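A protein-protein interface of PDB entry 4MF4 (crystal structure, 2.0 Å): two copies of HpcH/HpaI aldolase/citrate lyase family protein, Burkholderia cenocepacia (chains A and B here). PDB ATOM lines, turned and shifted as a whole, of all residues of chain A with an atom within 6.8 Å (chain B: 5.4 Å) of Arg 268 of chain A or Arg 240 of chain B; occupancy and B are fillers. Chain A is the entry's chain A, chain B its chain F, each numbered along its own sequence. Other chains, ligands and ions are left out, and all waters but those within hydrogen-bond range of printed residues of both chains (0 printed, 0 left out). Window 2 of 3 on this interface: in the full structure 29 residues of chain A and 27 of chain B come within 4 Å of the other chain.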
ATOM      1  N   ALA A 263     -18.409  -5.266  33.237  1.00  0.00           N
ATOM      2  CA  ALA A 263     -18.178  -5.237  31.788  1.00  0.00           C
ATOM      3  C   ALA A 263     -17.143  -4.178  31.352  1.00  0.00           C
ATOM      4  O   ALA A 263     -16.201  -4.465  30.566  1.00  0.00           O
ATOM      5  CB  ALA A 263     -19.491  -5.060  31.080  1.00  0.00           C
ATOM      6  N   LEU A 264     -17.243  -2.995  31.935  1.00  0.00           N
ATOM      7  CA  LEU A 264     -16.291  -1.912  31.670  1.00  0.00           C
ATOM      8  C   LEU A 264     -14.867  -2.325  32.043  1.00  0.00           C
ATOM      9  O   LEU A 264     -13.920  -2.148  31.253  1.00  0.00           O
ATOM     10  CB  LEU A 264     -16.666  -0.661  32.465  1.00  0.00           C
ATOM     11  CG  LEU A 264     -15.869   0.578  32.127  1.00  0.00           C
ATOM     12  CD1 LEU A 264     -15.865   0.809  30.626  1.00  0.00           C
ATOM     13  CD2 LEU A 264     -16.449   1.765  32.869  1.00  0.00           C
ATOM     14  N   GLN A 265     -14.720  -2.904  33.224  1.00  0.00           N
ATOM     15  CA  GLN A 265     -13.424  -3.383  33.646  1.00  0.00           C
ATOM     16  C   GLN A 265     -12.866  -4.433  32.686  1.00  0.00           C
ATOM     17  O   GLN A 265     -11.683  -4.429  32.380  1.00  0.00           O
ATOM     18  CB  GLN A 265     -13.497  -3.981  35.034  1.00  0.00           C
ATOM     19  CG  GLN A 265     -12.150  -4.570  35.460  1.00  0.00           C
ATOM     20  CD  GLN A 265     -12.187  -5.067  36.880  1.00  0.00           C
ATOM     21  OE1 GLN A 265     -12.791  -6.101  37.180  1.00  0.00           O
ATOM     22  NE2 GLN A 265     -11.564  -4.317  37.773  1.00  0.00           N
ATOM     23  N   GLU A 266     -13.705  -5.369  32.277  1.00  0.00           N
ATOM     24  CA  GLU A 266     -13.270  -6.426  31.374  1.00  0.00           C
ATOM     25  C   GLU A 266     -12.816  -5.900  30.021  1.00  0.00           C
ATOM     26  O   GLU A 266     -11.842  -6.375  29.451  1.00  0.00           O
ATOM     27  CB  GLU A 266     -14.383  -7.439  31.162  1.00  0.00           C
ATOM     28  CG  GLU A 266     -14.485  -8.446  32.295  1.00  0.00           C
ATOM     29  CD  GLU A 266     -15.678  -9.354  32.115  1.00  0.00           C
ATOM     30  OE1 GLU A 266     -16.058  -9.565  30.939  1.00  0.00           O
ATOM     31  OE2 GLU A 266     -16.226  -9.852  33.125  1.00  0.00           O
ATOM     32  N   VAL A 267     -13.535  -4.926  29.503  1.00  0.00           N
ATOM     33  CA  VAL A 267     -13.226  -4.382  28.208  1.00  0.00           C
ATOM     34  C   VAL A 267     -11.929  -3.570  28.250  1.00  0.00           C
ATOM     35  O   VAL A 267     -11.204  -3.538  27.269  1.00  0.00           O
ATOM     36  CB  VAL A 267     -14.387  -3.504  27.713  1.00  0.00           C
ATOM     37  CG1 VAL A 267     -13.968  -2.616  26.574  1.00  0.00           C
ATOM     38  CG2 VAL A 267     -15.567  -4.375  27.300  1.00  0.00           C
ATOM     39  N   ARG A 268     -11.673  -2.915  29.376  1.00  0.00           N
ATOM     40  CA  ARG A 268     -10.453  -2.126  29.596  1.00  0.00           C
ATOM     41  C   ARG A 268      -9.205  -2.896  29.986  1.00  0.00           C
ATOM     42  O   ARG A 268      -8.114  -2.355  29.905  1.00  0.00           O
ATOM     43  CB  ARG A 268     -10.670  -1.181  30.751  1.00  0.00           C
ATOM     44  CG  ARG A 268     -11.236   0.132  30.362  1.00  0.00           C
ATOM     45  CD  ARG A 268     -11.553   0.842  31.644  1.00  0.00           C
ATOM     46  NE  ARG A 268     -12.051   2.160  31.360  1.00  0.00           N
ATOM     47  CZ  ARG A 268     -12.719   2.899  32.233  1.00  0.00           C
ATOM     48  NH1 ARG A 268     -12.957   2.438  33.464  1.00  0.00           N
ATOM     49  NH2 ARG A 268     -13.151   4.101  31.866  1.00  0.00           N
ATOM     50  N   SER A 269      -9.351  -4.122  30.466  1.00  0.00           N
ATOM     51  CA  SER A 269      -8.206  -4.858  30.983  1.00  0.00           C
ATOM     52  C   SER A 269      -7.306  -5.370  29.860  1.00  0.00           C
ATOM     53  O   SER A 269      -7.434  -4.999  28.698  1.00  0.00           O
ATOM     54  CB  SER A 269      -8.678  -6.031  31.825  1.00  0.00           C
ATOM     55  OG  SER A 269      -9.238  -7.023  30.978  1.00  0.00           O
ATOM     56  OXT SER A 269      -6.415  -6.185  30.100  1.00  0.00           O
ATOM     57  N   PRO B  26      -9.717   4.966  23.494  1.00  0.00           N
ATOM     58  CA  PRO B  26     -11.102   4.570  23.253  1.00  0.00           C
ATOM     59  C   PRO B  26     -12.054   5.337  24.207  1.00  0.00           C
ATOM     60  O   PRO B  26     -11.617   5.884  25.194  1.00  0.00           O
ATOM     61  CB  PRO B  26     -11.089   3.081  23.548  1.00  0.00           C
ATOM     62  CG  PRO B  26      -9.971   2.866  24.505  1.00  0.00           C
ATOM     63  CD  PRO B  26      -8.993   3.990  24.334  1.00  0.00           C
ATOM     64  N   TYR B  28     -15.615   4.660  26.050  1.00  0.00           N
ATOM     65  CA  TYR B  28     -16.556   3.574  26.269  1.00  0.00           C
ATOM     66  C   TYR B  28     -17.914   4.110  26.710  1.00  0.00           C
ATOM     67  O   TYR B  28     -18.002   4.979  27.599  1.00  0.00           O
ATOM     68  CB  TYR B  28     -16.010   2.608  27.310  1.00  0.00           C
ATOM     69  CG  TYR B  28     -14.766   1.895  26.848  1.00  0.00           C
ATOM     70  CD1 TYR B  28     -14.851   0.947  25.844  1.00  0.00           C
ATOM     71  CD2 TYR B  28     -13.523   2.190  27.393  1.00  0.00           C
ATOM     72  CE1 TYR B  28     -13.722   0.297  25.365  1.00  0.00           C
ATOM     73  CE2 TYR B  28     -12.359   1.511  26.948  1.00  0.00           C
ATOM     74  CZ  TYR B  28     -12.491   0.579  25.927  1.00  0.00           C
ATOM     75  OH  TYR B  28     -11.413  -0.116  25.450  1.00  0.00           O
ATOM     76  N   GLY B  47     -18.947   4.790  35.735  1.00  0.00           N
ATOM     77  CA  GLY B  47     -17.570   5.036  35.268  1.00  0.00           C
ATOM     78  C   GLY B  47     -17.440   5.112  33.756  1.00  0.00           C
ATOM     79  O   GLY B  47     -16.345   5.191  33.274  1.00  0.00           O
ATOM     80  N   ASP B  49     -17.432   6.668  29.934  1.00  0.00           N
ATOM     81  CA  ASP B  49     -17.175   7.939  29.255  1.00  0.00           C
ATOM     82  C   ASP B  49     -18.429   8.546  28.653  1.00  0.00           C
ATOM     83  O   ASP B  49     -18.530   9.750  28.602  1.00  0.00           O
ATOM     84  CB  ASP B  49     -16.111   7.735  28.194  1.00  0.00           C
ATOM     85  CG  ASP B  49     -14.826   7.158  28.782  1.00  0.00           C
ATOM     86  OD1 ASP B  49     -14.263   7.785  29.711  1.00  0.00           O
ATOM     87  OD2 ASP B  49     -14.408   6.079  28.333  1.00  0.00           O
ATOM     88  N   ALA B 235     -16.557  -8.950  21.867  1.00  0.00           N
ATOM     89  CA  ALA B 235     -16.697  -8.090  20.710  1.00  0.00           C
ATOM     90  C   ALA B 235     -16.176  -6.674  20.964  1.00  0.00           C
ATOM     91  O   ALA B 235     -15.466  -6.104  20.150  1.00  0.00           O
ATOM     92  CB  ALA B 235     -18.154  -8.022  20.302  1.00  0.00           C
ATOM     93  N   ALA B 236     -16.505  -6.104  22.108  1.00  0.00           N
ATOM     94  CA  ALA B 236     -15.974  -4.781  22.420  1.00  0.00           C
ATOM     95  C   ALA B 236     -14.441  -4.825  22.382  1.00  0.00           C
ATOM     96  O   ALA B 236     -13.787  -3.921  21.826  1.00  0.00           O
ATOM     97  CB  ALA B 236     -16.481  -4.307  23.764  1.00  0.00           C
ATOM     98  N   ARG B 237     -13.859  -5.884  22.940  1.00  0.00           N
ATOM     99  CA  ARG B 237     -12.392  -5.963  22.960  1.00  0.00           C
ATOM    100  C   ARG B 237     -11.839  -6.102  21.542  1.00  0.00           C
ATOM    101  O   ARG B 237     -10.857  -5.440  21.214  1.00  0.00           O
ATOM    102  CB  ARG B 237     -11.898  -7.086  23.856  1.00  0.00           C
ATOM    103  CG  ARG B 237     -12.221  -6.850  25.347  1.00  0.00           C
ATOM    104  CD  ARG B 237     -11.718  -7.973  26.253  1.00  0.00           C
ATOM    105  NE  ARG B 237     -10.274  -8.174  26.083  1.00  0.00           N
ATOM    106  CZ  ARG B 237      -9.314  -7.452  26.661  1.00  0.00           C
ATOM    107  NH1 ARG B 237      -9.605  -6.469  27.510  1.00  0.00           N
ATOM    108  NH2 ARG B 237      -8.040  -7.734  26.404  1.00  0.00           N
ATOM    109  N   GLN B 238     -12.479  -6.925  20.705  1.00  0.00           N
ATOM    110  CA  GLN B 238     -12.072  -7.066  19.294  1.00  0.00           C
ATOM    111  C   GLN B 238     -12.069  -5.680  18.637  1.00  0.00           C
ATOM    112  O   GLN B 238     -11.110  -5.293  17.980  1.00  0.00           O
ATOM    113  CB  GLN B 238     -13.016  -8.004  18.539  1.00  0.00           C
ATOM    114  N   TYR B 239     -13.133  -4.904  18.868  1.00  0.00           N
ATOM    115  CA  TYR B 239     -13.257  -3.600  18.223  1.00  0.00           C
ATOM    116  C   TYR B 239     -12.183  -2.635  18.674  1.00  0.00           C
ATOM    117  O   TYR B 239     -11.616  -1.883  17.859  1.00  0.00           O
ATOM    118  CB  TYR B 239     -14.678  -3.034  18.443  1.00  0.00           C
ATOM    119  CG  TYR B 239     -15.800  -3.920  17.898  1.00  0.00           C
ATOM    120  CD1 TYR B 239     -15.587  -4.786  16.831  1.00  0.00           C
ATOM    121  CD2 TYR B 239     -17.080  -3.851  18.419  1.00  0.00           C
ATOM    122  CE1 TYR B 239     -16.601  -5.571  16.323  1.00  0.00           C
ATOM    123  CE2 TYR B 239     -18.121  -4.627  17.907  1.00  0.00           C
ATOM    124  CZ  TYR B 239     -17.885  -5.493  16.875  1.00  0.00           C
ATOM    125  OH  TYR B 239     -18.906  -6.284  16.363  1.00  0.00           O
ATOM    126  N   ARG B 240     -11.907  -2.623  19.973  1.00  0.00           N
ATOM    127  CA  ARG B 240     -10.853  -1.776  20.494  1.00  0.00           C
ATOM    128  C   ARG B 240      -9.504  -2.125  19.803  1.00  0.00           C
ATOM    129  O   ARG B 240      -8.776  -1.229  19.415  1.00  0.00           O
ATOM    130  CB  ARG B 240     -10.692  -1.898  22.015  1.00  0.00           C
ATOM    131  CG  ARG B 240      -9.354  -1.286  22.478  1.00  0.00           C
ATOM    132  CD  ARG B 240      -9.080  -1.194  23.976  1.00  0.00           C
ATOM    133  NE  ARG B 240      -9.055  -2.485  24.664  1.00  0.00           N
ATOM    134  CZ  ARG B 240      -8.301  -2.778  25.737  1.00  0.00           C
ATOM    135  NH1 ARG B 240      -7.482  -1.890  26.292  1.00  0.00           N
ATOM    136  NH2 ARG B 240      -8.358  -3.992  26.267  1.00  0.00           N
ATOM    137  N   GLU B 241      -9.194  -3.415  19.682  1.00  0.00           N
ATOM    138  CA  GLU B 241      -7.915  -3.862  19.111  1.00  0.00           C
ATOM    139  C   GLU B 241      -7.883  -3.457  17.649  1.00  0.00           C
ATOM    140  O   GLU B 241      -6.822  -3.172  17.127  1.00  0.00           O
ATOM    141  CB  GLU B 241      -7.726  -5.380  19.282  1.00  0.00           C
ATOM    142  N   ALA B 242      -9.053  -3.375  17.008  1.00  0.00           N
ATOM    143  CA  ALA B 242      -9.112  -3.050  15.584  1.00  0.00           C
ATOM    144  C   ALA B 242      -8.962  -1.565  15.300  1.00  0.00           C
ATOM    145  O   ALA B 242      -8.695  -1.182  14.171  1.00  0.00           O
ATOM    146  CB  ALA B 242     -10.394  -3.584  14.961  1.00  0.00           C
ATOM    147  N   GLY B 243      -9.149  -0.723  16.306  1.00  0.00           N
ATOM    148  CA  GLY B 243      -8.993   0.725  16.132  1.00  0.00           C
ATOM    149  C   GLY B 243     -10.261   1.557  16.289  1.00  0.00           C
ATOM    150  O   GLY B 243     -10.230   2.779  16.132  1.00  0.00           O
ATOM    151  N   TYR B 244     -11.386   0.920  16.607  1.00  0.00           N
ATOM    152  CA  TYR B 244     -12.608   1.690  16.918  1.00  0.00           C
ATOM    153  C   TYR B 244     -12.347   2.477  18.178  1.00  0.00           C
ATOM    154  O   TYR B 244     -11.665   1.987  19.078  1.00  0.00           O
ATOM    155  CB  TYR B 244     -13.781   0.758  17.140  1.00  0.00           C
ATOM    156  CG  TYR B 244     -14.249   0.094  15.866  1.00  0.00           C
ATOM    157  CD1 TYR B 244     -15.195   0.707  15.054  1.00  0.00           C
ATOM    158  CD2 TYR B 244     -13.771  -1.166  15.476  1.00  0.00           C
ATOM    159  CE1 TYR B 244     -15.640   0.092  13.884  1.00  0.00           C
ATOM    160  CE2 TYR B 244     -14.207  -1.771  14.301  1.00  0.00           C
ATOM    161  CZ  TYR B 244     -15.152  -1.131  13.519  1.00  0.00           C
ATOM    162  OH  TYR B 244     -15.612  -1.708  12.336  1.00  0.00           O
ATOM    163  N   ILE B 247     -16.864   3.116  21.573  1.00  0.00           N
ATOM    164  CA  ILE B 247     -17.361   1.743  21.646  1.00  0.00           C
ATOM    165  C   ILE B 247     -18.512   1.642  22.665  1.00  0.00           C
ATOM    166  O   ILE B 247     -18.378   1.941  23.878  1.00  0.00           O
ATOM    167  CB  ILE B 247     -16.203   0.760  21.967  1.00  0.00           C
ATOM    168  CG1 ILE B 247     -15.102   0.849  20.897  1.00  0.00           C
ATOM    169  CG2 ILE B 247     -16.690  -0.688  22.023  1.00  0.00           C
ATOM    170  CD1 ILE B 247     -13.828   0.120  21.282  1.00  0.00           C
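The backbone carbonyl oxygen (O) of Val 267 of chain A sits at hydrogen-bond distance from the guanidinium group (NH2) of Arg 240 of chain B (3.1 Å).
O of Val 267 of chain A lies within hydrogen-bond range of NH1 of Arg 237 of chain B, at 3.3 Å.
The guanidinium group of Arg 240 of chain B is in salt-bridge range of the chain-end carboxylate of Ser 269 of chain A, 2.8 Å away.
The chain-end carboxylate (O) of Ser 269 of chain A lies within salt-bridge range of the guanidinium group (NH1) of Arg 237 of chain B (2.9 Å).
The backbone carbonyl oxygen (O) of Glu 266 of chain A sits at hydrogen-bond distance from the guanidinium group (NH1) of Arg 237 of chain B (3.0 Å).
OH of Tyr 28 of chain B lies close to NE of Arg 240 of chain B.
The backbone carbonyl oxygen of Tyr 28 of chain B lies within hydrogen-bond range of the backbone NH of Asp 49 of chain B (2.9 Å).
O of Glu 266 of chain A sits at hydrogen-bond distance from OG of Ser 269 of chain A (3.1 Å).
Leu 264 of chain A touches Tyr 28 of chain B.
Leu 264 of chain A touches Gly 47 of chain B (CD2 to O, 3.5 Å).
Val 267 of chain A touches Tyr 28 of chain B (CG1 to CE1, 3.2 Å).
Val 267 of chain A touches Ala 236 of chain B.
Tyr 28 of chain B touches Arg 268 of chain A.
O of Gly 47 of chain B touches NH2 of Arg 268 of chain A, at 3.7 Å.
Arg 268 of chain A touches Arg 240 of chain B.
Arg 268 of chain A touches just these residues of chain B: Tyr 28 (3.8 Å), Gly 47 (3.7 Å) and Arg 240 (3.7 Å).
Printed residues of chain B within 4 Å of Val 267 of chain A: Tyr 28, Ala 236, Arg 237 and Arg 240.
Of the printed residues of chain A, Ala 236 of chain B touches Val 267.
Asp 49 of chain B touches none of the printed residues of chain A.
Gln 238 of chain B touches none of the printed residues of chain A.
The nearest residue of chain A that does not touch Arg 240 of chain B is Glu 266 of chain A (5.3 Å).
Printed residues of chain A that touch a printed residue of chain B: Leu 264, Glu 266, Val 267, Arg 268 and Ser 269.
Hydrophobic or aromatic side chains of chain A that line the printed part of chain B: Leu 264 and Val 267.
Hydrophobic or aromatic side chains of chain B within 4 Å of the printed part of chain A: Tyr 28 and Ala 236.
No position is printed for both chains.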
